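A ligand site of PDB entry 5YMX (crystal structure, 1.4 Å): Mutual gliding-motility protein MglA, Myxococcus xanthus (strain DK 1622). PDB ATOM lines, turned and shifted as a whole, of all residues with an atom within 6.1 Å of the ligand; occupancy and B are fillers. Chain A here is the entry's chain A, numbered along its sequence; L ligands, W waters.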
ATOM      1  N   GLY A  19     -14.386   0.599 -22.373  1.00  0.00           N
ATOM      2  CA  GLY A  19     -13.902  -0.745 -22.212  1.00  0.00           C
ATOM      3  C   GLY A  19     -13.855  -1.454 -23.553  1.00  0.00           C
ATOM      4  O   GLY A  19     -14.338  -0.924 -24.556  1.00  0.00           O
ATOM      5  N   PRO A  20     -13.285  -2.657 -23.591  1.00  0.00           N
ATOM      6  CA  PRO A  20     -13.119  -3.331 -24.889  1.00  0.00           C
ATOM      7  C   PRO A  20     -14.457  -3.675 -25.529  1.00  0.00           C
ATOM      8  O   PRO A  20     -15.508  -3.702 -24.879  1.00  0.00           O
ATOM      9  CB  PRO A  20     -12.335  -4.606 -24.555  1.00  0.00           C
ATOM     10  CG  PRO A  20     -12.281  -4.706 -23.085  1.00  0.00           C
ATOM     11  CD  PRO A  20     -12.762  -3.440 -22.466  1.00  0.00           C
ATOM     12  N   GLY A  21     -14.409  -3.928 -26.824  1.00  0.00           N
ATOM     13  CA  GLY A  21     -15.609  -4.350 -27.513  1.00  0.00           C
ATOM     14  C   GLY A  21     -16.239  -5.554 -26.849  1.00  0.00           C
ATOM     15  O   GLY A  21     -15.537  -6.472 -26.409  1.00  0.00           O
ATOM     16  N   LEU A  22     -17.573  -5.547 -26.748  1.00  0.00           N
ATOM     17  CA  LEU A  22     -18.357  -6.682 -26.272  1.00  0.00           C
ATOM     18  C   LEU A  22     -18.172  -6.963 -24.794  1.00  0.00           C
ATOM     19  O   LEU A  22     -18.473  -8.073 -24.334  1.00  0.00           O
ATOM     20  CB  LEU A  22     -18.123  -7.954 -27.107  1.00  0.00           C
ATOM     21  CG  LEU A  22     -18.248  -7.778 -28.617  1.00  0.00           C
ATOM     22  CD1 LEU A  22     -17.982  -9.074 -29.366  1.00  0.00           C
ATOM     23  CD2 LEU A  22     -19.622  -7.237 -28.984  1.00  0.00           C
ATOM     24  N   CYS A  23     -17.690  -5.986 -24.030  1.00  0.00           N
ATOM     25  CA  CYS A  23     -17.467  -6.193 -22.610  1.00  0.00           C
ATOM     26  C   CYS A  23     -18.703  -5.995 -21.754  1.00  0.00           C
ATOM     27  O   CYS A  23     -18.666  -6.386 -20.581  1.00  0.00           O
ATOM     28  CB  CYS A  23     -16.336  -5.294 -22.109  1.00  0.00           C
ATOM     29  SG  CYS A  23     -16.744  -3.536 -22.109  1.00  0.00           S
ATOM     30  N   GLY A  24     -19.770  -5.377 -22.282  1.00  0.00           N
ATOM     31  CA  GLY A  24     -20.977  -5.166 -21.521  1.00  0.00           C
ATOM     32  C   GLY A  24     -21.453  -3.733 -21.384  1.00  0.00           C
ATOM     33  O   GLY A  24     -22.305  -3.460 -20.538  1.00  0.00           O
ATOM     34  N   LYS A  25     -20.928  -2.797 -22.184  1.00  0.00           N
ATOM     35  CA  LYS A  25     -21.298  -1.393 -22.027  1.00  0.00           C
ATOM     36  C   LYS A  25     -22.752  -1.136 -22.438  1.00  0.00           C
ATOM     37  O   LYS A  25     -23.509  -0.514 -21.700  1.00  0.00           O
ATOM     38  CB  LYS A  25     -20.318  -0.511 -22.806  1.00  0.00           C
ATOM     39  CG  LYS A  25     -18.879  -0.740 -22.353  1.00  0.00           C
ATOM     40  CD  LYS A  25     -17.830   0.120 -23.059  1.00  0.00           C
ATOM     41  CE  LYS A  25     -17.770  -0.092 -24.559  1.00  0.00           C
ATOM     42  NZ  LYS A  25     -17.454  -1.513 -24.936  1.00  0.00           N
ATOM     43  N   THR A  26     -23.135  -1.619 -23.616  1.00  0.00           N
ATOM     44  CA  THR A  26     -24.537  -1.524 -24.034  1.00  0.00           C
ATOM     45  C   THR A  26     -25.457  -2.127 -22.988  1.00  0.00           C
ATOM     46  O   THR A  26     -26.504  -1.545 -22.656  1.00  0.00           O
ATOM     47  CB  THR A  26     -24.748  -2.273 -25.365  1.00  0.00           C
ATOM     48  OG1 THR A  26     -23.951  -1.674 -26.392  1.00  0.00           O
ATOM     49  CG2 THR A  26     -26.238  -2.233 -25.786  1.00  0.00           C
ATOM     50  N   THR A  27     -25.080  -3.294 -22.462  1.00  0.00           N
ATOM     51  CA  THR A  27     -25.937  -3.981 -21.503  1.00  0.00           C
ATOM     52  C   THR A  27     -26.127  -3.144 -20.244  1.00  0.00           C
ATOM     53  O   THR A  27     -27.239  -3.045 -19.724  1.00  0.00           O
ATOM     54  CB  THR A  27     -25.339  -5.366 -21.186  1.00  0.00           C
ATOM     55  OG1 THR A  27     -25.153  -6.097 -22.404  1.00  0.00           O
ATOM     56  CG2 THR A  27     -26.265  -6.157 -20.286  1.00  0.00           C
ATOM     57  N   ASN A  28     -25.049  -2.528 -19.756  1.00  0.00           N
ATOM     58  CA  ASN A  28     -25.179  -1.596 -18.642  1.00  0.00           C
ATOM     59  C   ASN A  28     -26.165  -0.486 -18.968  1.00  0.00           C
ATOM     60  O   ASN A  28     -27.080  -0.199 -18.181  1.00  0.00           O
ATOM     61  CB  ASN A  28     -23.815  -0.978 -18.313  1.00  0.00           C
ATOM     62  CG  ASN A  28     -23.032  -1.770 -17.274  1.00  0.00           C
ATOM     63  OD1 ASN A  28     -23.146  -1.503 -16.092  1.00  0.00           O
ATOM     64  ND2 ASN A  28     -22.231  -2.743 -17.736  1.00  0.00           N
ATOM     65  N   GLN A  30     -28.539  -0.208 -21.238  1.00  0.00           N
ATOM     66  CA  GLN A  30     -29.908  -0.667 -21.441  1.00  0.00           C
ATOM     67  C   GLN A  30     -30.557  -1.055 -20.123  1.00  0.00           C
ATOM     68  O   GLN A  30     -31.747  -0.774 -19.911  1.00  0.00           O
ATOM     69  CB  GLN A  30     -29.920  -1.881 -22.377  1.00  0.00           C
ATOM     70  CG  GLN A  30     -29.646  -1.596 -23.837  1.00  0.00           C
ATOM     71  CD  GLN A  30     -29.477  -2.879 -24.630  1.00  0.00           C
ATOM     72  OE1 GLN A  30     -29.053  -3.905 -24.092  1.00  0.00           O
ATOM     73  NE2 GLN A  30     -29.795  -2.826 -25.910  1.00  0.00           N
ATOM     74  N   THR A  78     -21.598   5.750 -24.556  1.00  0.00           N
ATOM     75  CA  THR A  78     -20.631   4.708 -24.842  1.00  0.00           C
ATOM     76  C   THR A  78     -20.487   4.540 -26.344  1.00  0.00           C
ATOM     77  O   THR A  78     -21.372   4.913 -27.123  1.00  0.00           O
ATOM     78  CB  THR A  78     -21.030   3.379 -24.178  1.00  0.00           C
ATOM     79  OG1 THR A  78     -19.881   2.526 -24.087  1.00  0.00           O
ATOM     80  CG2 THR A  78     -22.128   2.628 -24.945  1.00  0.00           C
ATOM     81  N   VAL A  79     -19.351   3.968 -26.740  1.00  0.00           N
ATOM     82  CA  VAL A  79     -19.124   3.516 -28.119  1.00  0.00           C
ATOM     83  C   VAL A  79     -19.213   1.999 -28.068  1.00  0.00           C
ATOM     84  O   VAL A  79     -18.270   1.349 -27.607  1.00  0.00           O
ATOM     85  CB  VAL A  79     -17.753   3.955 -28.643  1.00  0.00           C
ATOM     86  CG1 VAL A  79     -17.491   3.357 -30.013  1.00  0.00           C
ATOM     87  CG2 VAL A  79     -17.660   5.460 -28.688  1.00  0.00           C
ATOM     88  N   PRO A  80     -20.323   1.411 -28.480  1.00  0.00           N
ATOM     89  CA  PRO A  80     -20.520  -0.031 -28.281  1.00  0.00           C
ATOM     90  C   PRO A  80     -19.933  -0.850 -29.427  1.00  0.00           C
ATOM     91  O   PRO A  80     -19.749  -0.360 -30.546  1.00  0.00           O
ATOM     92  CB  PRO A  80     -22.050  -0.160 -28.284  1.00  0.00           C
ATOM     93  CG  PRO A  80     -22.480   0.899 -29.242  1.00  0.00           C
ATOM     94  CD  PRO A  80     -21.528   2.058 -29.036  1.00  0.00           C
ATOM     95  N   GLY A  81     -19.662  -2.105 -29.118  1.00  0.00           N
ATOM     96  CA  GLY A  81     -19.299  -3.076 -30.128  1.00  0.00           C
ATOM     97  C   GLY A  81     -17.862  -2.950 -30.580  1.00  0.00           C
ATOM     98  O   GLY A  81     -17.021  -2.283 -29.948  1.00  0.00           O
ATOM     99  N   GLN A  82     -17.563  -3.613 -31.692  1.00  0.00           N
ATOM    100  CA  GLN A  82     -16.232  -3.493 -32.268  1.00  0.00           C
ATOM    101  C   GLN A  82     -16.012  -2.059 -32.739  1.00  0.00           C
ATOM    102  O   GLN A  82     -16.872  -1.452 -33.383  1.00  0.00           O
ATOM    103  CB  GLN A  82     -16.092  -4.450 -33.448  1.00  0.00           C
ATOM    104  CG  GLN A  82     -14.738  -4.387 -34.120  1.00  0.00           C
ATOM    105  CD  GLN A  82     -14.566  -5.441 -35.192  1.00  0.00           C
ATOM    106  OE1 GLN A  82     -15.467  -6.256 -35.435  1.00  0.00           O
ATOM    107  NE2 GLN A  82     -13.407  -5.444 -35.845  1.00  0.00           N
ATOM    108  N   ASN A 141     -17.113  -7.007 -15.016  1.00  0.00           N
ATOM    109  CA  ASN A 141     -18.366  -7.549 -15.528  1.00  0.00           C
ATOM    110  C   ASN A 141     -18.188  -9.019 -15.920  1.00  0.00           C
ATOM    111  O   ASN A 141     -17.072  -9.530 -16.057  1.00  0.00           O
ATOM    112  CB  ASN A 141     -18.863  -6.696 -16.709  1.00  0.00           C
ATOM    113  CG  ASN A 141     -20.279  -7.042 -17.103  1.00  0.00           C
ATOM    114  OD1 ASN A 141     -21.121  -7.341 -16.253  1.00  0.00           O
ATOM    115  ND2 ASN A 141     -20.548  -7.013 -18.408  1.00  0.00           N
ATOM    116  N   LYS A 142     -19.314  -9.709 -16.130  1.00  0.00           N
ATOM    117  CA  LYS A 142     -19.328 -11.118 -16.538  1.00  0.00           C
ATOM    118  C   LYS A 142     -18.798 -12.023 -15.435  1.00  0.00           C
ATOM    119  O   LYS A 142     -18.167 -13.053 -15.708  1.00  0.00           O
ATOM    120  CB  LYS A 142     -18.598 -11.349 -17.879  1.00  0.00           C
ATOM    121  CG  LYS A 142     -18.963 -10.334 -18.964  1.00  0.00           C
ATOM    122  CD  LYS A 142     -18.651 -10.849 -20.363  1.00  0.00           C
ATOM    123  CE  LYS A 142     -19.041  -9.863 -21.434  1.00  0.00           C
ATOM    124  NZ  LYS A 142     -18.625 -10.322 -22.786  1.00  0.00           N
ATOM    125  N   ARG A 143     -19.092 -11.667 -14.174  1.00  0.00           N
ATOM    126  CA  ARG A 143     -18.667 -12.501 -13.053  1.00  0.00           C
ATOM    127  C   ARG A 143     -19.320 -13.882 -13.088  1.00  0.00           C
ATOM    128  O   ARG A 143     -18.844 -14.784 -12.390  1.00  0.00           O
ATOM    129  CB  ARG A 143     -19.010 -11.823 -11.726  1.00  0.00           C
ATOM    130  CG  ARG A 143     -18.432 -10.416 -11.534  1.00  0.00           C
ATOM    131  CD  ARG A 143     -16.919 -10.374 -11.755  1.00  0.00           C
ATOM    132  NE  ARG A 143     -16.227 -11.263 -10.832  1.00  0.00           N
ATOM    133  CZ  ARG A 143     -15.035 -11.800 -11.050  1.00  0.00           C
ATOM    134  NH1 ARG A 143     -14.398 -11.540 -12.189  1.00  0.00           N
ATOM    135  NH2 ARG A 143     -14.481 -12.615 -10.164  1.00  0.00           N
ATOM    136  N   ASP A 144     -20.380 -14.056 -13.875  1.00  0.00           N
ATOM    137  CA  ASP A 144     -21.110 -15.316 -13.939  1.00  0.00           C
ATOM    138  C   ASP A 144     -20.382 -16.388 -14.736  1.00  0.00           C
ATOM    139  O   ASP A 144     -20.682 -17.572 -14.583  1.00  0.00           O
ATOM    140  CB  ASP A 144     -22.480 -15.089 -14.582  1.00  0.00           C
ATOM    141  CG  ASP A 144     -22.380 -14.499 -15.984  1.00  0.00           C
ATOM    142  OD1 ASP A 144     -21.736 -13.437 -16.145  1.00  0.00           O
ATOM    143  OD2 ASP A 144     -22.929 -15.093 -16.928  1.00  0.00           O
ATOM    144  N   LEU A 145     -19.423 -16.017 -15.570  1.00  0.00           N
ATOM    145  CA  LEU A 145     -18.867 -16.995 -16.499  1.00  0.00           C
ATOM    146  C   LEU A 145     -17.780 -17.829 -15.819  1.00  0.00           C
ATOM    147  O   LEU A 145     -17.022 -17.324 -15.001  1.00  0.00           O
ATOM    148  CB  LEU A 145     -18.301 -16.308 -17.728  1.00  0.00           C
ATOM    149  CG  LEU A 145     -19.337 -15.632 -18.635  1.00  0.00           C
ATOM    150  CD1 LEU A 145     -18.663 -14.868 -19.773  1.00  0.00           C
ATOM    151  CD2 LEU A 145     -20.326 -16.694 -19.158  1.00  0.00           C
ATOM    152  N   ALA A 168     -20.023  -7.210 -11.453  1.00  0.00           N
ATOM    153  CA  ALA A 168     -21.296  -7.083 -12.155  1.00  0.00           C
ATOM    154  C   ALA A 168     -21.593  -8.320 -12.999  1.00  0.00           C
ATOM    155  O   ALA A 168     -20.690  -9.024 -13.455  1.00  0.00           O
ATOM    156  CB  ALA A 168     -21.345  -5.827 -13.047  1.00  0.00           C
ATOM    157  N   VAL A 169     -22.894  -8.561 -13.183  1.00  0.00           N
ATOM    158  CA  VAL A 169     -23.410  -9.444 -14.218  1.00  0.00           C
ATOM    159  C   VAL A 169     -24.448  -8.585 -14.944  1.00  0.00           C
ATOM    160  O   VAL A 169     -25.617  -8.541 -14.572  1.00  0.00           O
ATOM    161  CB  VAL A 169     -24.045 -10.718 -13.654  1.00  0.00           C
ATOM    162  CG1 VAL A 169     -24.549 -11.605 -14.787  1.00  0.00           C
ATOM    163  CG2 VAL A 169     -23.029 -11.456 -12.795  1.00  0.00           C
ATOM    164  N   ALA A 170     -23.993  -7.826 -15.936  1.00  0.00           N
ATOM    165  CA  ALA A 170     -24.839  -6.753 -16.450  1.00  0.00           C
ATOM    166  C   ALA A 170     -26.200  -7.212 -16.949  1.00  0.00           C
ATOM    167  O   ALA A 170     -27.181  -6.482 -16.721  1.00  0.00           O
ATOM    168  CB  ALA A 170     -24.072  -5.950 -17.511  1.00  0.00           C
ATOM    169  N   PRO A 171     -26.353  -8.364 -17.620  1.00  0.00           N
ATOM    170  CA  PRO A 171     -27.671  -8.708 -18.163  1.00  0.00           C
ATOM    171  C   PRO A 171     -28.741  -8.882 -17.105  1.00  0.00           C
ATOM    172  O   PRO A 171     -29.927  -8.675 -17.398  1.00  0.00           O
ATOM    173  CB  PRO A 171     -27.417  -9.996 -18.958  1.00  0.00           C
ATOM    174  CG  PRO A 171     -25.947  -9.935 -19.284  1.00  0.00           C
ATOM    175  CD  PRO A 171     -25.310  -9.306 -18.075  1.00  0.00           C
HETATM  176  P1  LIG L   1     -20.457  -3.615 -25.607  1.00  0.00           P
HETATM  177  O1  LIG L   1     -21.592  -2.631 -25.638  1.00  0.00           O
HETATM  178  O2  LIG L   1     -19.827  -3.824 -26.952  1.00  0.00           O
HETATM  179  O3  LIG L   1     -19.445  -3.336 -24.547  1.00  0.00           O
HETATM  180  O4  LIG L   1     -21.052  -5.075 -25.192  1.00  0.00           O
HETATM  181  P2  LIG L   1     -22.577  -5.559 -24.970  1.00  0.00           P
HETATM  182  O5  LIG L   1     -23.310  -5.463 -26.280  1.00  0.00           O
HETATM  183  O6  LIG L   1     -23.206  -4.905 -23.781  1.00  0.00           O
HETATM  184  O7  LIG L   1     -22.348  -7.101 -24.596  1.00  0.00           O
HETATM  185  C1  LIG L   1     -21.766  -8.017 -25.521  1.00  0.00           C
HETATM  186  C2  LIG L   1     -22.305  -9.419 -25.256  1.00  0.00           C
HETATM  187  O8  LIG L   1     -21.913  -9.858 -23.949  1.00  0.00           O
HETATM  188  C3  LIG L   1     -23.816  -9.515 -25.297  1.00  0.00           C
HETATM  189  O9  LIG L   1     -24.157 -10.790 -25.858  1.00  0.00           O
HETATM  190  C4  LIG L   1     -24.215  -9.471 -23.835  1.00  0.00           C
HETATM  191  O10 LIG L   1     -25.456 -10.132 -23.592  1.00  0.00           O
HETATM  192  C5  LIG L   1     -23.069 -10.230 -23.192  1.00  0.00           C
HETATM  193  N1  LIG L   1     -22.867  -9.845 -21.796  1.00  0.00           N
HETATM  194  C6  LIG L   1     -22.751  -8.580 -21.306  1.00  0.00           C
HETATM  195  N2  LIG L   1     -22.564  -8.612 -19.963  1.00  0.00           N
HETATM  196  C7  LIG L   1     -22.507  -9.921 -19.607  1.00  0.00           C
HETATM  197  C8  LIG L   1     -22.331 -10.656 -18.353  1.00  0.00           C
HETATM  198  O11 LIG L   1     -22.160 -10.059 -17.280  1.00  0.00           O
HETATM  199  N3  LIG L   1     -22.360 -11.992 -18.420  1.00  0.00           N
HETATM  200  C9  LIG L   1     -22.545 -12.691 -19.544  1.00  0.00           C
HETATM  201  N4  LIG L   1     -22.552 -14.039 -19.486  1.00  0.00           N
HETATM  202  N5  LIG L   1     -22.716 -12.083 -20.753  1.00  0.00           N
HETATM  203  C10 LIG L   1     -22.705 -10.727 -20.815  1.00  0.00           C
HETATM  204  O   HOH W   1     -25.836  -6.071 -26.881  1.00  0.00           O
HETATM  205  O   HOH W   2     -22.145 -13.066 -25.106  1.00  0.00           O
HETATM  206  O   HOH W   3     -21.986  -4.753 -28.592  1.00  0.00           O
HETATM  207  O   HOH W   4     -22.961  -9.237 -28.718  1.00  0.00           O
HETATM  208  O   HOH W   5     -25.260 -13.365 -22.180  1.00  0.00           O
HETATM  209  O   HOH W   6     -20.134 -12.725 -23.073  1.00  0.00           O
HETATM  210  O   HOH W   7     -22.693 -15.824 -22.057  1.00  0.00           O
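The backbone NH (N) of Thr 26 lies within hydrogen-bond range of an oxygen (O1) of the ligand. An oxygen (O3) of the ligand lies within hydrogen-bond range of the side-chain sulfur (SG) of Cys 23 (3.6 Å). N of Leu 22 is in hydrogen-bond range of O2 of the ligand (2.8 Å). An oxygen (O2) of the ligand sits at hydrogen-bond distance from the backbone NH (N) of Gly 81, at 2.8 Å. O3 of the ligand is in salt-bridge range of NZ of Lys 25, at 2.7 Å. O11 of the ligand lies within hydrogen-bond range of N of Lys 142 (3.1 Å). An oxygen (O11) of the ligand is in hydrogen-bond range of the backbone NH of Ala 170, at 3.2 Å. The side-chain hydroxyl (OG1) of Thr 26 is in hydrogen-bond range of an oxygen (O1) of the ligand (2.7 Å). The side-chain amide nitrogen of Asn 141 sits at hydrogen-bond distance from a nitrogen (N2) of the ligand (3.0 Å). O3 of the ligand lies within hydrogen-bond range of N of Lys 25, at 2.8 Å. The backbone NH (N) of Gly 24 lies within hydrogen-bond range of an oxygen (O3) of the ligand. N of Thr 27 lies within hydrogen-bond range of O6 of the ligand, at 2.8 Å. An oxygen (O6) of the ligand lies within hydrogen-bond range of the side-chain hydroxyl of Thr 27, 2.7 Å away. N3 of the ligand sits at hydrogen-bond distance from OD1 of Asp 144 (2.8 Å). The backbone NH of Cys 23 sits at hydrogen-bond distance from an oxygen (O3) of the ligand, at 3.2 Å.
The backbone NH of Lys 142 is in hydrogen-bond range of the backbone carbonyl oxygen of Ala 168. The side-chain amide oxygen (OD1) of Asn 141 is in hydrogen-bond range of the backbone NH (N) of Ala 170. SG of Cys 23 sits at hydrogen-bond distance from O of Pro 20. O of Cys 23 sits at hydrogen-bond distance from ND2 of Asn 141 (2.9 Å). The backbone carbonyl oxygen (O) of Leu 22 sits at hydrogen-bond distance from the side-chain amino group (NZ) of Lys 142, at 2.7 Å. The side-chain amino group (NZ) of Lys 25 is in hydrogen-bond range of the backbone carbonyl oxygen (O) of Pro 20 (2.9 Å). SG of Cys 23 sits close to NZ of Lys 25 (3.5 Å). OD1 of Asn 141 lies close to O of Ala 168 (3.3 Å).
Merely in contact with the ligand: Pro 20 (3.97 Å), Gly 21 (3.98 Å), Pro 80 (3.6 Å), Leu 145 (3.5 Å), Val 169 (3.4 Å) and Pro 171 (3.3 Å). 17 residues have an atom within 4 Å of the ligand: Pro 20, Gly 21, Leu 22, Cys 23, Gly 24, Lys 25, Thr 26, Thr 27, Pro 80, Gly 81, Asn 141, Lys 142, Asp 144, Leu 145, Val 169, Ala 170 and Pro 171. The nearest printed residue that does not touch the ligand is Ala 168 (4.2 Å).
Water W6 bridges NZ of Lys 142 (2.9 Å) and O8 of the ligand (3.5 Å).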
